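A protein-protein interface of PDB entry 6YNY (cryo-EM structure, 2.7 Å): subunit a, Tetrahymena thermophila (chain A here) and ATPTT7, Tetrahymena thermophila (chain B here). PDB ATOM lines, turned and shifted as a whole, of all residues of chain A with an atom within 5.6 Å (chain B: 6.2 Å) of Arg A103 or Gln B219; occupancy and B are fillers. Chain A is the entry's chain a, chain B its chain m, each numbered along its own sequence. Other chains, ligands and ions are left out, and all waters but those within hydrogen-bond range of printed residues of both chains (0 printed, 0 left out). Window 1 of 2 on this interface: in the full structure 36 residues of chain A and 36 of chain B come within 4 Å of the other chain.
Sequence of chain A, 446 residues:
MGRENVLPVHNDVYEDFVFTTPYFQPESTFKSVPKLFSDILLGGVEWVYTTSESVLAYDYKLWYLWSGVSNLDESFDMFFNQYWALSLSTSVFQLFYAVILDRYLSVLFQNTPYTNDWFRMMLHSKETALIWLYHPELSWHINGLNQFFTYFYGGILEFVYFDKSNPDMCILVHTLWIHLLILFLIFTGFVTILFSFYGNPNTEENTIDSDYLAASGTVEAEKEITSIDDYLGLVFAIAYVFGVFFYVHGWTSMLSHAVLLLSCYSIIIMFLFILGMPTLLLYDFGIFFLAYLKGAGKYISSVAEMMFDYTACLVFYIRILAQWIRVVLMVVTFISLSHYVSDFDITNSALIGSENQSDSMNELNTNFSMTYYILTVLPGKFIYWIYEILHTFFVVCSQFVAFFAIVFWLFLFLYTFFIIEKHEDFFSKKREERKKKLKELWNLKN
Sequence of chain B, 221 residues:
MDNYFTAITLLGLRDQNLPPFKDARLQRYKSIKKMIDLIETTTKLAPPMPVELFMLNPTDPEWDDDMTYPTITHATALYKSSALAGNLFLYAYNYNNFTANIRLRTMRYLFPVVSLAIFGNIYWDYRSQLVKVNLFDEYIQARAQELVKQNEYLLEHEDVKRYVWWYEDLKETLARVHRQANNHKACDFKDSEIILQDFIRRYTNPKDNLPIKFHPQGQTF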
ATOM      1  N   ALA A  98      28.847  16.302  -3.614  1.00  0.00           N
ATOM      2  CA  ALA A  98      29.666  15.148  -3.956  1.00  0.00           C
ATOM      3  C   ALA A  98      29.387  14.678  -5.375  1.00  0.00           C
ATOM      4  O   ALA A  98      30.306  14.276  -6.096  1.00  0.00           O
ATOM      5  CB  ALA A  98      29.416  14.023  -2.959  1.00  0.00           C
ATOM      6  N   VAL A  99      28.121  14.717  -5.791  1.00  0.00           N
ATOM      7  CA  VAL A  99      27.766  14.305  -7.141  1.00  0.00           C
ATOM      8  C   VAL A  99      28.298  15.298  -8.161  1.00  0.00           C
ATOM      9  O   VAL A  99      28.695  14.912  -9.266  1.00  0.00           O
ATOM     10  CB  VAL A  99      26.239  14.141  -7.243  1.00  0.00           C
ATOM     11  CG1 VAL A  99      25.822  13.838  -8.664  1.00  0.00           C
ATOM     12  CG2 VAL A  99      25.772  13.048  -6.309  1.00  0.00           C
ATOM     13  N   ILE A 100      28.320  16.584  -7.815  1.00  0.00           N
ATOM     14  CA  ILE A 100      28.854  17.592  -8.722  1.00  0.00           C
ATOM     15  C   ILE A 100      30.345  17.381  -8.939  1.00  0.00           C
ATOM     16  O   ILE A 100      30.856  17.556 -10.050  1.00  0.00           O
ATOM     17  CB  ILE A 100      28.560  19.000  -8.177  1.00  0.00           C
ATOM     18  CG1 ILE A 100      27.060  19.271  -8.164  1.00  0.00           C
ATOM     19  CG2 ILE A 100      29.281  20.043  -8.987  1.00  0.00           C
ATOM     20  CD1 ILE A 100      26.399  19.168  -9.504  1.00  0.00           C
ATOM     21  N   LEU A 101      31.066  17.010  -7.882  1.00  0.00           N
ATOM     22  CA  LEU A 101      32.498  16.772  -8.010  1.00  0.00           C
ATOM     23  C   LEU A 101      32.784  15.524  -8.831  1.00  0.00           C
ATOM     24  O   LEU A 101      33.712  15.510  -9.647  1.00  0.00           O
ATOM     25  CB  LEU A 101      33.127  16.651  -6.625  1.00  0.00           C
ATOM     26  CG  LEU A 101      33.189  17.930  -5.801  1.00  0.00           C
ATOM     27  CD1 LEU A 101      33.515  17.607  -4.371  1.00  0.00           C
ATOM     28  CD2 LEU A 101      34.224  18.870  -6.370  1.00  0.00           C
ATOM     29  N   ASP A 102      31.999  14.467  -8.630  1.00  0.00           N
ATOM     30  CA  ASP A 102      32.199  13.245  -9.396  1.00  0.00           C
ATOM     31  C   ASP A 102      31.893  13.446 -10.871  1.00  0.00           C
ATOM     32  O   ASP A 102      32.457  12.746 -11.718  1.00  0.00           O
ATOM     33  CB  ASP A 102      31.334  12.128  -8.822  1.00  0.00           C
ATOM     34  CG  ASP A 102      31.767  11.716  -7.432  1.00  0.00           C
ATOM     35  OD1 ASP A 102      32.968  11.845  -7.123  1.00  0.00           O
ATOM     36  OD2 ASP A 102      30.907  11.262  -6.651  1.00  0.00           O
ATOM     37  N   ARG A 103      31.005  14.381 -11.201  1.00  0.00           N
ATOM     38  CA  ARG A 103      30.749  14.689 -12.600  1.00  0.00           C
ATOM     39  C   ARG A 103      31.816  15.606 -13.176  1.00  0.00           C
ATOM     40  O   ARG A 103      32.070  15.573 -14.383  1.00  0.00           O
ATOM     41  CB  ARG A 103      29.370  15.323 -12.748  1.00  0.00           C
ATOM     42  CG  ARG A 103      28.232  14.406 -12.367  1.00  0.00           C
ATOM     43  CD  ARG A 103      28.040  13.291 -13.369  1.00  0.00           C
ATOM     44  NE  ARG A 103      27.679  13.797 -14.688  1.00  0.00           N
ATOM     45  CZ  ARG A 103      27.266  13.033 -15.692  1.00  0.00           C
ATOM     46  NH1 ARG A 103      27.156  11.723 -15.532  1.00  0.00           N
ATOM     47  NH2 ARG A 103      26.957  13.581 -16.858  1.00  0.00           N
ATOM     48  N   TYR A 104      32.444  16.424 -12.334  1.00  0.00           N
ATOM     49  CA  TYR A 104      33.556  17.247 -12.787  1.00  0.00           C
ATOM     50  C   TYR A 104      34.765  16.393 -13.138  1.00  0.00           C
ATOM     51  O   TYR A 104      35.507  16.724 -14.069  1.00  0.00           O
ATOM     52  CB  TYR A 104      33.911  18.265 -11.707  1.00  0.00           C
ATOM     53  CG  TYR A 104      35.117  19.114 -12.017  1.00  0.00           C
ATOM     54  CD1 TYR A 104      35.026  20.187 -12.884  1.00  0.00           C
ATOM     55  CD2 TYR A 104      36.345  18.850 -11.432  1.00  0.00           C
ATOM     56  CE1 TYR A 104      36.120  20.965 -13.167  1.00  0.00           C
ATOM     57  CE2 TYR A 104      37.443  19.624 -11.711  1.00  0.00           C
ATOM     58  CZ  TYR A 104      37.326  20.680 -12.578  1.00  0.00           C
ATOM     59  OH  TYR A 104      38.425  21.455 -12.857  1.00  0.00           O
ATOM     60  N   LEU A 105      34.975  15.298 -12.409  1.00  0.00           N
ATOM     61  CA  LEU A 105      36.074  14.394 -12.718  1.00  0.00           C
ATOM     62  C   LEU A 105      35.817  13.604 -13.993  1.00  0.00           C
ATOM     63  O   LEU A 105      36.767  13.233 -14.690  1.00  0.00           O
ATOM     64  CB  LEU A 105      36.306  13.443 -11.549  1.00  0.00           C
ATOM     65  CG  LEU A 105      36.763  14.090 -10.244  1.00  0.00           C
ATOM     66  CD1 LEU A 105      36.915  13.039  -9.177  1.00  0.00           C
ATOM     67  CD2 LEU A 105      38.058  14.846 -10.433  1.00  0.00           C
ATOM     68  N   SER A 106      34.553  13.336 -14.314  1.00  0.00           N
ATOM     69  CA  SER A 106      34.230  12.657 -15.558  1.00  0.00           C
ATOM     70  C   SER A 106      34.392  13.560 -16.769  1.00  0.00           C
ATOM     71  O   SER A 106      34.392  13.062 -17.899  1.00  0.00           O
ATOM     72  CB  SER A 106      32.804  12.121 -15.505  1.00  0.00           C
ATOM     73  OG  SER A 106      31.872  13.181 -15.440  1.00  0.00           O
ATOM     74  N   VAL A 107      34.519  14.867 -16.557  1.00  0.00           N
ATOM     75  CA  VAL A 107      34.770  15.793 -17.653  1.00  0.00           C
ATOM     76  C   VAL A 107      36.258  15.871 -17.961  1.00  0.00           C
ATOM     77  O   VAL A 107      36.668  15.816 -19.126  1.00  0.00           O
ATOM     78  CB  VAL A 107      34.192  17.175 -17.311  1.00  0.00           C
ATOM     79  CG1 VAL A 107      34.685  18.203 -18.293  1.00  0.00           C
ATOM     80  CG2 VAL A 107      32.683  17.117 -17.307  1.00  0.00           C
ATOM     81  N   SER A 139      28.079  20.562 -16.429  1.00  0.00           N
ATOM     82  CA  SER A 139      28.820  19.334 -16.679  1.00  0.00           C
ATOM     83  C   SER A 139      28.045  18.406 -17.603  1.00  0.00           C
ATOM     84  O   SER A 139      28.636  17.720 -18.444  1.00  0.00           O
ATOM     85  CB  SER A 139      29.131  18.632 -15.361  1.00  0.00           C
ATOM     86  OG  SER A 139      27.949  18.167 -14.741  1.00  0.00           O
ATOM     87  N   TRP A 140      26.721  18.369 -17.461  1.00  0.00           N
ATOM     88  CA  TRP A 140      25.908  17.518 -18.319  1.00  0.00           C
ATOM     89  C   TRP A 140      25.844  18.065 -19.737  1.00  0.00           C
ATOM     90  O   TRP A 140      25.869  17.298 -20.706  1.00  0.00           O
ATOM     91  CB  TRP A 140      24.507  17.377 -17.733  1.00  0.00           C
ATOM     92  CG  TRP A 140      24.465  16.573 -16.483  1.00  0.00           C
ATOM     93  CD1 TRP A 140      24.294  15.229 -16.387  1.00  0.00           C
ATOM     94  CD2 TRP A 140      24.596  17.057 -15.146  1.00  0.00           C
ATOM     95  NE1 TRP A 140      24.312  14.843 -15.075  1.00  0.00           N
ATOM     96  CE2 TRP A 140      24.498  15.947 -14.291  1.00  0.00           C
ATOM     97  CE3 TRP A 140      24.790  18.321 -14.586  1.00  0.00           C
ATOM     98  CZ2 TRP A 140      24.582  16.061 -12.911  1.00  0.00           C
ATOM     99  CZ3 TRP A 140      24.876  18.430 -13.217  1.00  0.00           C
ATOM    100  CH2 TRP A 140      24.771  17.308 -12.394  1.00  0.00           C
ATOM    101  N   HIS A 141      25.757  19.387 -19.880  1.00  0.00           N
ATOM    102  CA  HIS A 141      25.756  19.989 -21.206  1.00  0.00           C
ATOM    103  C   HIS A 141      27.015  19.633 -21.981  1.00  0.00           C
ATOM    104  O   HIS A 141      26.971  19.486 -23.207  1.00  0.00           O
ATOM    105  CB  HIS A 141      25.621  21.502 -21.090  1.00  0.00           C
ATOM    106  CG  HIS A 141      25.690  22.214 -22.401  1.00  0.00           C
ATOM    107  ND1 HIS A 141      24.752  22.037 -23.394  1.00  0.00           N
ATOM    108  CD2 HIS A 141      26.587  23.104 -22.885  1.00  0.00           C
ATOM    109  CE1 HIS A 141      25.068  22.789 -24.432  1.00  0.00           C
ATOM    110  NE2 HIS A 141      26.178  23.445 -24.150  1.00  0.00           N
ATOM    111  N   ASN A 143      29.124  16.826 -21.374  1.00  0.00           N
ATOM    112  CA  ASN A 143      29.186  15.395 -21.631  1.00  0.00           C
ATOM    113  C   ASN A 143      28.339  15.007 -22.833  1.00  0.00           C
ATOM    114  O   ASN A 143      28.661  14.044 -23.537  1.00  0.00           O
ATOM    115  CB  ASN A 143      28.737  14.631 -20.388  1.00  0.00           C
ATOM    116  CG  ASN A 143      29.031  13.153 -20.473  1.00  0.00           C
ATOM    117  OD1 ASN A 143      30.006  12.672 -19.897  1.00  0.00           O
ATOM    118  ND2 ASN A 143      28.194  12.422 -21.196  1.00  0.00           N
ATOM    119  N   GLY A 144      27.260  15.741 -23.085  1.00  0.00           N
ATOM    120  CA  GLY A 144      26.426  15.499 -24.241  1.00  0.00           C
ATOM    121  C   GLY A 144      27.014  16.117 -25.486  1.00  0.00           C
ATOM    122  O   GLY A 144      26.918  15.562 -26.583  1.00  0.00           O
ATOM    123  N   GLN A 147      29.758  13.986 -26.740  1.00  0.00           N
ATOM    124  CA  GLN A 147      29.188  12.791 -27.342  1.00  0.00           C
ATOM    125  C   GLN A 147      28.535  13.088 -28.683  1.00  0.00           C
ATOM    126  O   GLN A 147      28.525  12.227 -29.568  1.00  0.00           O
ATOM    127  CB  GLN A 147      28.178  12.166 -26.385  1.00  0.00           C
ATOM    128  CG  GLN A 147      27.459  10.957 -26.926  1.00  0.00           C
ATOM    129  CD  GLN A 147      26.703  10.208 -25.857  1.00  0.00           C
ATOM    130  OE1 GLN A 147      27.253   9.875 -24.809  1.00  0.00           O
ATOM    131  NE2 GLN A 147      25.432   9.941 -26.112  1.00  0.00           N
ATOM    132  N   GLU B  40      23.856   7.019 -10.157  1.00  0.00           N
ATOM    133  CA  GLU B  40      24.432   6.954 -11.494  1.00  0.00           C
ATOM    134  C   GLU B  40      23.361   7.112 -12.562  1.00  0.00           C
ATOM    135  O   GLU B  40      23.586   7.775 -13.581  1.00  0.00           O
ATOM    136  CB  GLU B  40      25.173   5.635 -11.683  1.00  0.00           C
ATOM    137  CG  GLU B  40      26.550   5.601 -11.062  1.00  0.00           C
ATOM    138  CD  GLU B  40      27.227   4.255 -11.225  1.00  0.00           C
ATOM    139  OE1 GLU B  40      26.531   3.271 -11.548  1.00  0.00           O
ATOM    140  OE2 GLU B  40      28.459   4.181 -11.037  1.00  0.00           O
ATOM    141  N   THR B  43      22.022  10.722 -13.042  1.00  0.00           N
ATOM    142  CA  THR B  43      22.944  11.580 -13.773  1.00  0.00           C
ATOM    143  C   THR B  43      22.918  11.347 -15.274  1.00  0.00           C
ATOM    144  O   THR B  43      23.588  12.082 -16.006  1.00  0.00           O
ATOM    145  CB  THR B  43      24.360  11.370 -13.247  1.00  0.00           C
ATOM    146  OG1 THR B  43      24.669   9.972 -13.241  1.00  0.00           O
ATOM    147  CG2 THR B  43      24.475  11.909 -11.851  1.00  0.00           C
ATOM    148  N   LYS B  44      22.168  10.354 -15.751  1.00  0.00           N
ATOM    149  CA  LYS B  44      22.076  10.049 -17.173  1.00  0.00           C
ATOM    150  C   LYS B  44      20.709  10.394 -17.746  1.00  0.00           C
ATOM    151  O   LYS B  44      20.312   9.837 -18.773  1.00  0.00           O
ATOM    152  CB  LYS B  44      22.392   8.573 -17.407  1.00  0.00           C
ATOM    153  CG  LYS B  44      23.810   8.194 -17.050  1.00  0.00           C
ATOM    154  CD  LYS B  44      23.966   6.707 -16.924  1.00  0.00           C
ATOM    155  CE  LYS B  44      25.348   6.342 -16.422  1.00  0.00           C
ATOM    156  NZ  LYS B  44      25.452   4.889 -16.100  1.00  0.00           N
ATOM    157  N   LEU B  45      19.986  11.309 -17.104  1.00  0.00           N
ATOM    158  CA  LEU B  45      18.658  11.718 -17.539  1.00  0.00           C
ATOM    159  C   LEU B  45      18.600  13.199 -17.876  1.00  0.00           C
ATOM    160  O   LEU B  45      17.504  13.745 -18.044  1.00  0.00           O
ATOM    161  CB  LEU B  45      17.629  11.390 -16.458  1.00  0.00           C
ATOM    162  CG  LEU B  45      17.659   9.949 -15.955  1.00  0.00           C
ATOM    163  CD1 LEU B  45      16.663   9.751 -14.844  1.00  0.00           C
ATOM    164  CD2 LEU B  45      17.392   8.977 -17.080  1.00  0.00           C
ATOM    165  N   ALA B  46      19.745  13.856 -17.983  1.00  0.00           N
ATOM    166  CA  ALA B  46      19.761  15.281 -18.241  1.00  0.00           C
ATOM    167  C   ALA B  46      19.260  15.573 -19.653  1.00  0.00           C
ATOM    168  O   ALA B  46      19.653  14.894 -20.606  1.00  0.00           O
ATOM    169  CB  ALA B  46      21.169  15.831 -18.069  1.00  0.00           C
ATOM    170  N   PRO B  47      18.399  16.570 -19.823  1.00  0.00           N
ATOM    171  CA  PRO B  47      17.918  16.909 -21.154  1.00  0.00           C
ATOM    172  C   PRO B  47      18.964  17.694 -21.923  1.00  0.00           C
ATOM    173  O   PRO B  47      19.863  18.302 -21.324  1.00  0.00           O
ATOM    174  CB  PRO B  47      16.676  17.760 -20.866  1.00  0.00           C
ATOM    175  CG  PRO B  47      16.963  18.388 -19.581  1.00  0.00           C
ATOM    176  CD  PRO B  47      17.787  17.423 -18.793  1.00  0.00           C
ATOM    177  N   ILE B 212      16.230   3.990 -20.883  1.00  0.00           N
ATOM    178  CA  ILE B 212      17.251   4.966 -21.240  1.00  0.00           C
ATOM    179  C   ILE B 212      17.528   4.809 -22.728  1.00  0.00           C
ATOM    180  O   ILE B 212      18.123   3.818 -23.158  1.00  0.00           O
ATOM    181  CB  ILE B 212      18.524   4.776 -20.412  1.00  0.00           C
ATOM    182  CG1 ILE B 212      18.232   5.018 -18.935  1.00  0.00           C
ATOM    183  CG2 ILE B 212      19.614   5.714 -20.899  1.00  0.00           C
ATOM    184  CD1 ILE B 212      19.343   4.609 -18.023  1.00  0.00           C
ATOM    185  N   HIS B 215      20.638   9.148 -27.605  1.00  0.00           N
ATOM    186  CA  HIS B 215      20.632  10.218 -28.571  1.00  0.00           C
ATOM    187  C   HIS B 215      22.010  10.865 -28.545  1.00  0.00           C
ATOM    188  O   HIS B 215      22.628  10.971 -27.476  1.00  0.00           O
ATOM    189  CB  HIS B 215      19.540  11.263 -28.296  1.00  0.00           C
ATOM    190  CG  HIS B 215      19.624  11.903 -26.949  1.00  0.00           C
ATOM    191  ND1 HIS B 215      20.030  13.207 -26.772  1.00  0.00           N
ATOM    192  CD2 HIS B 215      19.332  11.429 -25.717  1.00  0.00           C
ATOM    193  CE1 HIS B 215      19.994  13.506 -25.486  1.00  0.00           C
ATOM    194  NE2 HIS B 215      19.576  12.443 -24.823  1.00  0.00           N
ATOM    195  N   GLN B 217      23.267  13.599 -28.303  1.00  0.00           N
ATOM    196  CA  GLN B 217      23.496  14.659 -27.333  1.00  0.00           C
ATOM    197  C   GLN B 217      23.155  14.215 -25.916  1.00  0.00           C
ATOM    198  O   GLN B 217      22.798  15.041 -25.071  1.00  0.00           O
ATOM    199  CB  GLN B 217      22.686  15.893 -27.716  1.00  0.00           C
ATOM    200  CG  GLN B 217      23.230  17.188 -27.170  1.00  0.00           C
ATOM    201  CD  GLN B 217      22.517  18.392 -27.727  1.00  0.00           C
ATOM    202  OE1 GLN B 217      21.807  18.301 -28.728  1.00  0.00           O
ATOM    203  NE2 GLN B 217      22.694  19.530 -27.079  1.00  0.00           N
ATOM    204  N   GLY B 218      23.264  12.916 -25.642  1.00  0.00           N
ATOM    205  CA  GLY B 218      22.895  12.358 -24.363  1.00  0.00           C
ATOM    206  C   GLY B 218      24.092  12.069 -23.475  1.00  0.00           C
ATOM    207  O   GLY B 218      25.219  12.499 -23.724  1.00  0.00           O
ATOM    208  N   GLN B 219      23.825  11.311 -22.418  1.00  0.00           N
ATOM    209  CA  GLN B 219      24.794  11.033 -21.369  1.00  0.00           C
ATOM    210  C   GLN B 219      25.164   9.558 -21.390  1.00  0.00           C
ATOM    211  O   GLN B 219      24.285   8.692 -21.338  1.00  0.00           O
ATOM    212  CB  GLN B 219      24.232  11.402 -19.997  1.00  0.00           C
ATOM    213  CG  GLN B 219      23.834  12.851 -19.850  1.00  0.00           C
ATOM    214  CD  GLN B 219      25.019  13.775 -19.755  1.00  0.00           C
ATOM    215  OE1 GLN B 219      26.073  13.405 -19.240  1.00  0.00           O
ATOM    216  NE2 GLN B 219      24.855  14.989 -20.252  1.00  0.00           N
ATOM    217  N   THR B 220      26.461   9.280 -21.466  1.00  0.00           N
ATOM    218  CA  THR B 220      26.978   7.924 -21.366  1.00  0.00           C
ATOM    219  C   THR B 220      27.931   7.757 -20.195  1.00  0.00           C
ATOM    220  O   THR B 220      27.758   6.838 -19.387  1.00  0.00           O
ATOM    221  CB  THR B 220      27.681   7.528 -22.671  1.00  0.00           C
ATOM    222  OG1 THR B 220      26.728   7.486 -23.740  1.00  0.00           O
ATOM    223  CG2 THR B 220      28.329   6.176 -22.527  1.00  0.00           C
ATOM    224  N   PHE B 221      28.932   8.623 -20.077  1.00  0.00           N
ATOM    225  CA  PHE B 221      29.837   8.599 -18.939  1.00  0.00           C
ATOM    226  C   PHE B 221      29.332   9.522 -17.837  1.00  0.00           C
ATOM    227  O   PHE B 221      29.601   9.300 -16.656  1.00  0.00           O
ATOM    228  CB  PHE B 221      31.249   9.013 -19.362  1.00  0.00           C
ATOM    229  CG  PHE B 221      31.883   8.097 -20.368  1.00  0.00           C
ATOM    230  CD1 PHE B 221      32.836   8.580 -21.241  1.00  0.00           C
ATOM    231  CD2 PHE B 221      31.537   6.760 -20.441  1.00  0.00           C
ATOM    232  CE1 PHE B 221      33.430   7.751 -22.166  1.00  0.00           C
ATOM    233  CE2 PHE B 221      32.128   5.930 -21.365  1.00  0.00           C
ATOM    234  CZ  PHE B 221      33.076   6.426 -22.227  1.00  0.00           C
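The indole nitrogen (NE1) of Trp A140 is in hydrogen-bond range of the backbone carbonyl oxygen (O) of Thr B43 (3.0 Å). OE1 of Gln B219 sits at hydrogen-bond distance from ND2 of Asn A143. The side-chain amide nitrogen of Gln A147 is in hydrogen-bond range of the backbone carbonyl oxygen of His B215 (3.3 Å). NE2 of Gln B219 sits at hydrogen-bond distance from O of Trp A140 (2.6 Å). OG1 of Thr B220 lies within hydrogen-bond range of OE1 of Gln A147 (2.7 Å). The backbone carbonyl oxygen of Gly B218 sits close to the side-chain amide oxygen of Gln A147 (3.5 Å). The side-chain amide oxygen (OE1) of Gln B219 is in hydrogen-bond range of the guanidinium group (NH2) of Arg A103 (2.5 Å).
OG of Ser A106 sits at hydrogen-bond distance from O of Arg A103 (2.6 Å). ND1 of His B215 sits close to N of Gly B218 (3.4 Å). The backbone carbonyl oxygen (O) of Glu B40 lies within hydrogen-bond range of the side-chain hydroxyl (OG1) of Thr B43 (2.5 Å).
Among the printed residues, pairs that only touch across the chains: Gly A144 with Gly B218, Asn A143 with Thr B220, Trp A140 with Ala B46, Arg A103 with Thr B43, Gly A144 with Gln B217, Arg A103 with Phe B221, Asn A143 with Gly B218, Gly A144 with Gln B219, Asn A143 with Phe B221 and Val A99 with Thr B43.
Printed residues of chain B within 4 Å of Val A99: Thr B43. Arg A103 touches just these residues of chain B: Thr B43, Gln B219 and Phe B221. Of the printed residues of chain B, Trp A140 touches Thr B43 (3.0 Å), Ala B46 (3.6 Å) and Gln B219 (2.6 Å). Of the printed residues of chain B, Gln A147 touches His B215 (3.3 Å), Gly B218 (3.5 Å) and Thr B220 (2.7 Å). Pro B47 touches none of the printed residues of chain A. Printed residues of chain A within 4 Å of Gln B217: Gly A144. Of the printed residues of chain A, Gln B219 touches Arg A103 (2.5 Å), Trp A140 (2.6 Å), Asn A143 (3.0 Å) and Gly A144 (3.8 Å). The nearest residue of chain B that does not touch Arg A103 is Lys B44 (5.1 Å). The nearest printed residue of chain A that does not touch Gln B219 is Gln A147 (4.02 Å).
Of the 16 printed residues of chain A, 6 touch a printed residue of chain B. Hydrophobic or aromatic side chains of chain A that line the printed part of chain B: Val A99 and Trp A140. Among the printed residues, 17 pairs touch across the chains.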
